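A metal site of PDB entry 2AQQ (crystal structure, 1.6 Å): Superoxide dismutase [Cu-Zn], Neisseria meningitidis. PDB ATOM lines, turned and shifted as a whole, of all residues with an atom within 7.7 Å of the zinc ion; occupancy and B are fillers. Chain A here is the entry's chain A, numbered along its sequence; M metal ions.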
ATOM      1  N   PHE A  56     -22.651  -7.573  -0.136  1.00  0.00           N
ATOM      2  CA  PHE A  56     -23.875  -7.774   0.625  1.00  0.00           C
ATOM      3  C   PHE A  56     -23.485  -7.743   2.108  1.00  0.00           C
ATOM      4  O   PHE A  56     -22.834  -8.658   2.595  1.00  0.00           O
ATOM      5  CB  PHE A  56     -24.402  -9.156   0.215  1.00  0.00           C
ATOM      6  CG  PHE A  56     -25.846  -9.421   0.561  1.00  0.00           C
ATOM      7  CD1 PHE A  56     -26.821  -8.426   0.430  1.00  0.00           C
ATOM      8  CD2 PHE A  56     -26.244 -10.700   0.929  1.00  0.00           C
ATOM      9  CE1 PHE A  56     -28.162  -8.728   0.639  1.00  0.00           C
ATOM     10  CE2 PHE A  56     -27.583 -11.011   1.140  1.00  0.00           C
ATOM     11  CZ  PHE A  56     -28.548 -10.017   0.991  1.00  0.00           C
ATOM     12  N   HIS A  57     -23.862  -6.678   2.807  1.00  0.00           N
ATOM     13  CA  HIS A  57     -23.510  -6.551   4.222  1.00  0.00           C
ATOM     14  C   HIS A  57     -24.577  -5.896   5.090  1.00  0.00           C
ATOM     15  O   HIS A  57     -25.441  -5.174   4.598  1.00  0.00           O
ATOM     16  CB  HIS A  57     -22.234  -5.724   4.410  1.00  0.00           C
ATOM     17  CG  HIS A  57     -21.335  -5.686   3.220  1.00  0.00           C
ATOM     18  ND1 HIS A  57     -21.218  -4.571   2.413  1.00  0.00           N
ATOM     19  CD2 HIS A  57     -20.489  -6.610   2.711  1.00  0.00           C
ATOM     20  CE1 HIS A  57     -20.342  -4.816   1.454  1.00  0.00           C
ATOM     21  NE2 HIS A  57     -19.892  -6.049   1.608  1.00  0.00           N
ATOM     22  N   ILE A  58     -24.488  -6.143   6.391  1.00  0.00           N
ATOM     23  CA  ILE A  58     -25.401  -5.515   7.338  1.00  0.00           C
ATOM     24  C   ILE A  58     -24.676  -4.219   7.700  1.00  0.00           C
ATOM     25  O   ILE A  58     -23.487  -4.262   8.018  1.00  0.00           O
ATOM     26  CB  ILE A  58     -25.551  -6.322   8.643  1.00  0.00           C
ATOM     27  CG1 ILE A  58     -26.066  -7.740   8.332  1.00  0.00           C
ATOM     28  CG2 ILE A  58     -26.494  -5.585   9.605  1.00  0.00           C
ATOM     29  CD1 ILE A  58     -27.424  -7.772   7.664  1.00  0.00           C
ATOM     30  N   HIS A  59     -25.365  -3.082   7.617  1.00  0.00           N
ATOM     31  CA  HIS A  59     -24.744  -1.818   7.990  1.00  0.00           C
ATOM     32  C   HIS A  59     -25.304  -1.406   9.349  1.00  0.00           C
ATOM     33  O   HIS A  59     -26.397  -1.845   9.738  1.00  0.00           O
ATOM     34  CB  HIS A  59     -24.976  -0.753   6.924  1.00  0.00           C
ATOM     35  CG  HIS A  59     -24.063  -0.897   5.744  1.00  0.00           C
ATOM     36  ND1 HIS A  59     -23.230   0.120   5.317  1.00  0.00           N
ATOM     37  CD2 HIS A  59     -23.816  -1.954   4.935  1.00  0.00           C
ATOM     38  CE1 HIS A  59     -22.512  -0.304   4.291  1.00  0.00           C
ATOM     39  NE2 HIS A  59     -22.846  -1.560   4.038  1.00  0.00           N
ATOM     40  N   GLY A  81     -21.538   2.678   8.353  1.00  0.00           N
ATOM     41  CA  GLY A  81     -20.608   1.689   7.835  1.00  0.00           C
ATOM     42  C   GLY A  81     -21.051   0.267   8.064  1.00  0.00           C
ATOM     43  O   GLY A  81     -22.180   0.000   8.488  1.00  0.00           O
ATOM     44  N   HIS A  82     -20.159  -0.679   7.777  1.00  0.00           N
ATOM     45  CA  HIS A  82     -20.479  -2.088   7.972  1.00  0.00           C
ATOM     46  C   HIS A  82     -20.693  -2.294   9.467  1.00  0.00           C
ATOM     47  O   HIS A  82     -19.937  -1.767  10.281  1.00  0.00           O
ATOM     48  CB  HIS A  82     -19.323  -2.969   7.503  1.00  0.00           C
ATOM     49  CG  HIS A  82     -19.098  -2.935   6.016  1.00  0.00           C
ATOM     50  ND1 HIS A  82     -18.368  -3.906   5.359  1.00  0.00           N
ATOM     51  CD2 HIS A  82     -19.500  -2.058   5.073  1.00  0.00           C
ATOM     52  CE1 HIS A  82     -18.312  -3.614   4.073  1.00  0.00           C
ATOM     53  NE2 HIS A  82     -18.994  -2.502   3.867  1.00  0.00           N
ATOM     54  N   TRP A  83     -21.720  -3.053   9.826  1.00  0.00           N
ATOM     55  CA  TRP A  83     -21.988  -3.304  11.232  1.00  0.00           C
ATOM     56  C   TRP A  83     -20.784  -4.028  11.840  1.00  0.00           C
ATOM     57  O   TRP A  83     -20.409  -5.119  11.407  1.00  0.00           O
ATOM     58  CB  TRP A  83     -23.256  -4.135  11.384  1.00  0.00           C
ATOM     59  CG  TRP A  83     -23.714  -4.241  12.795  1.00  0.00           C
ATOM     60  CD1 TRP A  83     -23.739  -3.232  13.720  1.00  0.00           C
ATOM     61  CD2 TRP A  83     -24.206  -5.408  13.454  1.00  0.00           C
ATOM     62  NE1 TRP A  83     -24.225  -3.714  14.921  1.00  0.00           N
ATOM     63  CE2 TRP A  83     -24.516  -5.039  14.774  1.00  0.00           C
ATOM     64  CE3 TRP A  83     -24.417  -6.731  13.042  1.00  0.00           C
ATOM     65  CZ2 TRP A  83     -25.039  -5.949  15.703  1.00  0.00           C
ATOM     66  CZ3 TRP A  83     -24.934  -7.641  13.962  1.00  0.00           C
ATOM     67  CH2 TRP A  83     -25.237  -7.241  15.274  1.00  0.00           C
ATOM     68  N   ASP A  84     -20.189  -3.397  12.838  1.00  0.00           N
ATOM     69  CA  ASP A  84     -18.989  -3.931  13.477  1.00  0.00           C
ATOM     70  C   ASP A  84     -19.054  -3.770  14.998  1.00  0.00           C
ATOM     71  O   ASP A  84     -18.237  -3.062  15.591  1.00  0.00           O
ATOM     72  CB  ASP A  84     -17.787  -3.186  12.884  1.00  0.00           C
ATOM     73  CG  ASP A  84     -16.474  -3.738  13.358  1.00  0.00           C
ATOM     74  OD1 ASP A  84     -16.403  -4.937  13.696  1.00  0.00           O
ATOM     75  OD2 ASP A  84     -15.488  -2.971  13.356  1.00  0.00           O
ATOM     76  N   GLN A  90     -12.135  -4.215  10.336  1.00  0.00           N
ATOM     77  CA  GLN A  90     -11.527  -4.876   9.190  1.00  0.00           C
ATOM     78  C   GLN A  90     -12.624  -5.609   8.412  1.00  0.00           C
ATOM     79  O   GLN A  90     -13.466  -6.263   9.016  1.00  0.00           O
ATOM     80  CB  GLN A  90     -10.478  -5.867   9.688  1.00  0.00           C
ATOM     81  CG  GLN A  90      -9.901  -6.818   8.666  1.00  0.00           C
ATOM     82  CD  GLN A  90      -8.929  -7.797   9.292  1.00  0.00           C
ATOM     83  OE1 GLN A  90      -8.052  -7.405  10.050  1.00  0.00           O
ATOM     84  NE2 GLN A  90      -9.090  -9.075   8.977  1.00  0.00           N
ATOM     85  N   HIS A  91     -12.616  -5.478   7.087  1.00  0.00           N
ATOM     86  CA  HIS A  91     -13.600  -6.172   6.259  1.00  0.00           C
ATOM     87  C   HIS A  91     -13.029  -7.550   5.906  1.00  0.00           C
ATOM     88  O   HIS A  91     -11.849  -7.663   5.572  1.00  0.00           O
ATOM     89  CB  HIS A  91     -13.892  -5.387   4.987  1.00  0.00           C
ATOM     90  CG  HIS A  91     -14.922  -6.026   4.108  1.00  0.00           C
ATOM     91  ND1 HIS A  91     -16.250  -6.117   4.474  1.00  0.00           N
ATOM     92  CD2 HIS A  91     -14.810  -6.659   2.919  1.00  0.00           C
ATOM     93  CE1 HIS A  91     -16.911  -6.774   3.542  1.00  0.00           C
ATOM     94  NE2 HIS A  91     -16.068  -7.119   2.589  1.00  0.00           N
ATOM     95  N   GLY A  92     -13.860  -8.585   5.965  1.00  0.00           N
ATOM     96  CA  GLY A  92     -13.371  -9.915   5.645  1.00  0.00           C
ATOM     97  C   GLY A  92     -14.424 -10.897   5.171  1.00  0.00           C
ATOM     98  O   GLY A  92     -15.454 -10.499   4.619  1.00  0.00           O
ATOM     99  N   TYR A  93     -14.148 -12.181   5.386  1.00  0.00           N
ATOM    100  CA  TYR A  93     -15.039 -13.262   4.972  1.00  0.00           C
ATOM    101  C   TYR A  93     -16.190 -13.467   5.960  1.00  0.00           C
ATOM    102  O   TYR A  93     -16.092 -13.081   7.122  1.00  0.00           O
ATOM    103  CB  TYR A  93     -14.264 -14.574   4.851  1.00  0.00           C
ATOM    104  CG  TYR A  93     -13.253 -14.594   3.726  1.00  0.00           C
ATOM    105  CD1 TYR A  93     -13.655 -14.822   2.410  1.00  0.00           C
ATOM    106  CD2 TYR A  93     -11.898 -14.363   3.964  1.00  0.00           C
ATOM    107  CE1 TYR A  93     -12.737 -14.833   1.358  1.00  0.00           C
ATOM    108  CE2 TYR A  93     -10.978 -14.361   2.925  1.00  0.00           C
ATOM    109  CZ  TYR A  93     -11.404 -14.591   1.630  1.00  0.00           C
ATOM    110  OH  TYR A  93     -10.489 -14.590   0.599  1.00  0.00           O
ATOM    111  N   ALA A  99     -13.444 -10.152  11.390  1.00  0.00           N
ATOM    112  CA  ALA A  99     -13.951  -9.293  10.328  1.00  0.00           C
ATOM    113  C   ALA A  99     -15.274  -8.714  10.831  1.00  0.00           C
ATOM    114  O   ALA A  99     -15.853  -9.240  11.782  1.00  0.00           O
ATOM    115  CB  ALA A  99     -14.185 -10.106   9.068  1.00  0.00           C
ATOM    116  N   HIS A 100     -15.739  -7.641  10.208  1.00  0.00           N
ATOM    117  CA  HIS A 100     -17.013  -7.007  10.576  1.00  0.00           C
ATOM    118  C   HIS A 100     -18.068  -8.101  10.725  1.00  0.00           C
ATOM    119  O   HIS A 100     -18.193  -8.969   9.863  1.00  0.00           O
ATOM    120  CB  HIS A 100     -17.497  -6.056   9.469  1.00  0.00           C
ATOM    121  CG  HIS A 100     -16.529  -4.980   9.109  1.00  0.00           C
ATOM    122  ND1 HIS A 100     -16.317  -4.583   7.807  1.00  0.00           N
ATOM    123  CD2 HIS A 100     -15.763  -4.167   9.880  1.00  0.00           C
ATOM    124  CE1 HIS A 100     -15.473  -3.571   7.779  1.00  0.00           C
ATOM    125  NE2 HIS A 100     -15.114  -3.301   9.024  1.00  0.00           N
ATOM    126  N   LEU A 101     -18.865  -8.041  11.789  1.00  0.00           N
ATOM    127  CA  LEU A 101     -19.908  -9.042  11.991  1.00  0.00           C
ATOM    128  C   LEU A 101     -20.979  -8.943  10.898  1.00  0.00           C
ATOM    129  O   LEU A 101     -21.718  -9.896  10.651  1.00  0.00           O
ATOM    130  CB  LEU A 101     -20.554  -8.863  13.372  1.00  0.00           C
ATOM    131  CG  LEU A 101     -21.506  -9.980  13.788  1.00  0.00           C
ATOM    132  CD1 LEU A 101     -20.731 -11.294  13.876  1.00  0.00           C
ATOM    133  CD2 LEU A 101     -22.141  -9.640  15.128  1.00  0.00           C
ATOM    134  N   GLY A 102     -21.044  -7.787  10.240  1.00  0.00           N
ATOM    135  CA  GLY A 102     -22.024  -7.590   9.187  1.00  0.00           C
ATOM    136  C   GLY A 102     -21.628  -8.102   7.815  1.00  0.00           C
ATOM    137  O   GLY A 102     -22.390  -7.957   6.865  1.00  0.00           O
ATOM    138  N   ASP A 103     -20.452  -8.703   7.701  1.00  0.00           N
ATOM    139  CA  ASP A 103     -19.985  -9.199   6.404  1.00  0.00           C
ATOM    140  C   ASP A 103     -20.669 -10.503   5.996  1.00  0.00           C
ATOM    141  O   ASP A 103     -20.435 -11.560   6.578  1.00  0.00           O
ATOM    142  CB  ASP A 103     -18.457  -9.381   6.434  1.00  0.00           C
ATOM    143  CG  ASP A 103     -17.720  -8.058   6.595  1.00  0.00           C
ATOM    144  OD1 ASP A 103     -18.357  -6.999   6.381  1.00  0.00           O
ATOM    145  OD2 ASP A 103     -16.513  -8.077   6.911  1.00  0.00           O
ATOM    146  N   LEU A 104     -21.517 -10.407   4.974  1.00  0.00           N
ATOM    147  CA  LEU A 104     -22.270 -11.552   4.478  1.00  0.00           C
ATOM    148  C   LEU A 104     -21.684 -12.065   3.169  1.00  0.00           C
ATOM    149  O   LEU A 104     -20.863 -11.397   2.553  1.00  0.00           O
ATOM    150  CB  LEU A 104     -23.719 -11.147   4.215  1.00  0.00           C
ATOM    151  CG  LEU A 104     -24.464 -10.332   5.269  1.00  0.00           C
ATOM    152  CD1 LEU A 104     -25.815  -9.915   4.705  1.00  0.00           C
ATOM    153  CD2 LEU A 104     -24.629 -11.146   6.542  1.00  0.00           C
ATOM    154  N   ARG A 123     -21.660 -16.434  11.426  1.00  0.00           N
ATOM    155  CA  ARG A 123     -21.368 -15.706  12.651  1.00  0.00           C
ATOM    156  C   ARG A 123     -22.574 -14.994  13.255  1.00  0.00           C
ATOM    157  O   ARG A 123     -22.519 -14.557  14.403  1.00  0.00           O
ATOM    158  CB  ARG A 123     -20.215 -14.717  12.409  1.00  0.00           C
ATOM    159  CG  ARG A 123     -18.898 -15.420  12.147  1.00  0.00           C
ATOM    160  CD  ARG A 123     -17.768 -14.418  12.042  1.00  0.00           C
ATOM    161  NE  ARG A 123     -17.808 -13.677  10.789  1.00  0.00           N
ATOM    162  CZ  ARG A 123     -17.626 -12.367  10.700  1.00  0.00           C
ATOM    163  NH1 ARG A 123     -17.410 -11.644  11.789  1.00  0.00           N
ATOM    164  NH2 ARG A 123     -17.629 -11.776   9.504  1.00  0.00           N
ATOM    165  N   ASP A 142     -17.427  -8.213  -3.905  1.00  0.00           N
ATOM    166  CA  ASP A 142     -16.837  -8.346  -2.582  1.00  0.00           C
ATOM    167  C   ASP A 142     -15.720  -9.389  -2.587  1.00  0.00           C
ATOM    168  O   ASP A 142     -15.988 -10.596  -2.733  1.00  0.00           O
ATOM    169  CB  ASP A 142     -17.903  -8.766  -1.566  1.00  0.00           C
ATOM    170  CG  ASP A 142     -17.488  -8.498  -0.127  1.00  0.00           C
ATOM    171  OD1 ASP A 142     -16.269  -8.357   0.126  1.00  0.00           O
ATOM    172  OD2 ASP A 142     -18.364  -8.418   0.752  1.00  0.00           O
ATOM    173  N   HIS A 144     -13.870  -9.749  -0.061  1.00  0.00           N
ATOM    174  CA  HIS A 144     -13.714  -9.995   1.371  1.00  0.00           C
ATOM    175  C   HIS A 144     -12.389  -9.536   1.959  1.00  0.00           C
ATOM    176  O   HIS A 144     -11.825 -10.191   2.833  1.00  0.00           O
ATOM    177  CB  HIS A 144     -13.956 -11.477   1.657  1.00  0.00           C
ATOM    178  CG  HIS A 144     -15.341 -11.923   1.334  1.00  0.00           C
ATOM    179  ND1 HIS A 144     -16.456 -11.440   2.003  1.00  0.00           N
ATOM    180  CD2 HIS A 144     -15.820 -12.749   0.382  1.00  0.00           C
ATOM    181  CE1 HIS A 144     -17.548 -11.962   1.480  1.00  0.00           C
ATOM    182  NE2 HIS A 144     -17.191 -12.761   0.491  1.00  0.00           N
ATOM    183  N   SER A 145     -11.922  -8.379   1.493  1.00  0.00           N
ATOM    184  CA  SER A 145     -10.668  -7.816   1.982  1.00  0.00           C
ATOM    185  C   SER A 145     -10.703  -6.300   1.789  1.00  0.00           C
ATOM    186  O   SER A 145     -11.559  -5.772   1.072  1.00  0.00           O
ATOM    187  CB  SER A 145      -9.508  -8.409   1.190  1.00  0.00           C
ATOM    188  OG  SER A 145      -8.264  -7.869   1.604  1.00  0.00           O
ATOM    189  N   ASP A 146      -9.786  -5.603   2.441  1.00  0.00           N
ATOM    190  CA  ASP A 146      -9.703  -4.156   2.305  1.00  0.00           C
ATOM    191  C   ASP A 146      -8.620  -3.792   1.311  1.00  0.00           C
ATOM    192  O   ASP A 146      -8.191  -2.643   1.227  1.00  0.00           O
ATOM    193  CB  ASP A 146      -9.429  -3.497   3.660  1.00  0.00           C
ATOM    194  CG  ASP A 146     -10.636  -3.519   4.568  1.00  0.00           C
ATOM    195  OD1 ASP A 146     -11.692  -2.981   4.173  1.00  0.00           O
ATOM    196  OD2 ASP A 146     -10.535  -4.079   5.681  1.00  0.00           O
ATOM    197  N   LEU A 151     -13.259  -2.231   1.923  1.00  0.00           N
ATOM    198  CA  LEU A 151     -14.551  -2.873   2.059  1.00  0.00           C
ATOM    199  C   LEU A 151     -14.930  -3.836   0.923  1.00  0.00           C
ATOM    200  O   LEU A 151     -16.073  -3.853   0.472  1.00  0.00           O
ATOM    201  CB  LEU A 151     -15.616  -1.786   2.222  1.00  0.00           C
ATOM    202  CG  LEU A 151     -15.253  -0.780   3.324  1.00  0.00           C
ATOM    203  CD1 LEU A 151     -16.238   0.366   3.336  1.00  0.00           C
ATOM    204  CD2 LEU A 151     -15.232  -1.481   4.670  1.00  0.00           C
ATOM    205  N   GLY A 152     -13.953  -4.628   0.489  1.00  0.00           N
ATOM    206  CA  GLY A 152     -14.191  -5.608  -0.553  1.00  0.00           C
ATOM    207  C   GLY A 152     -14.432  -5.099  -1.955  1.00  0.00           C
ATOM    208  O   GLY A 152     -14.716  -5.884  -2.853  1.00  0.00           O
HETATM  209 ZN    ZN M   1     -17.251  -5.443   6.131  1.00  0.00          ZN
HETATM  210 CU    CU M   2     -22.061  -2.764   2.641  1.00  0.00          CU
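The nearest printed residue that does not touch the zinc ion is Gly 92 (4.6 Å).
The zinc ion is bound by the side-chain carboxylate of Asp 103 (1.9 Å), a ring nitrogen (ND1) of His 91 (2.0 Å), a ring nitrogen (ND1) of His 82 (2.1 Å) and a ring nitrogen (ND1) of His 100 (2.1 Å).
Slightly farther from the zinc ion lies the side-chain carboxylate (OD2) of Asp 103 (2.8 Å).
The backbone NH (N) of Gly 92 is in hydrogen-bond range of the side-chain carboxylate (OD2) of Asp 103.
A ring nitrogen (NE2) of His 91 sits at hydrogen-bond distance from the side-chain carboxylate (OD1) of Asp 142, 2.8 Å away.
The backbone NH (N) of His 91 sits at hydrogen-bond distance from the side-chain carboxylate (OD2) of Asp 146, at 2.9 Å.
NE2 of His 82 sits close to ND1 of His 57 (3.4 Å).
The backbone carbonyl oxygen (O) of Gln 90 is in hydrogen-bond range of the backbone NH (N) of His 100, 2.9 Å away.
The backbone carbonyl oxygen (O) of His 100 sits at hydrogen-bond distance from the guanidinium group (NH2) of Arg 123, 2.9 Å away.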
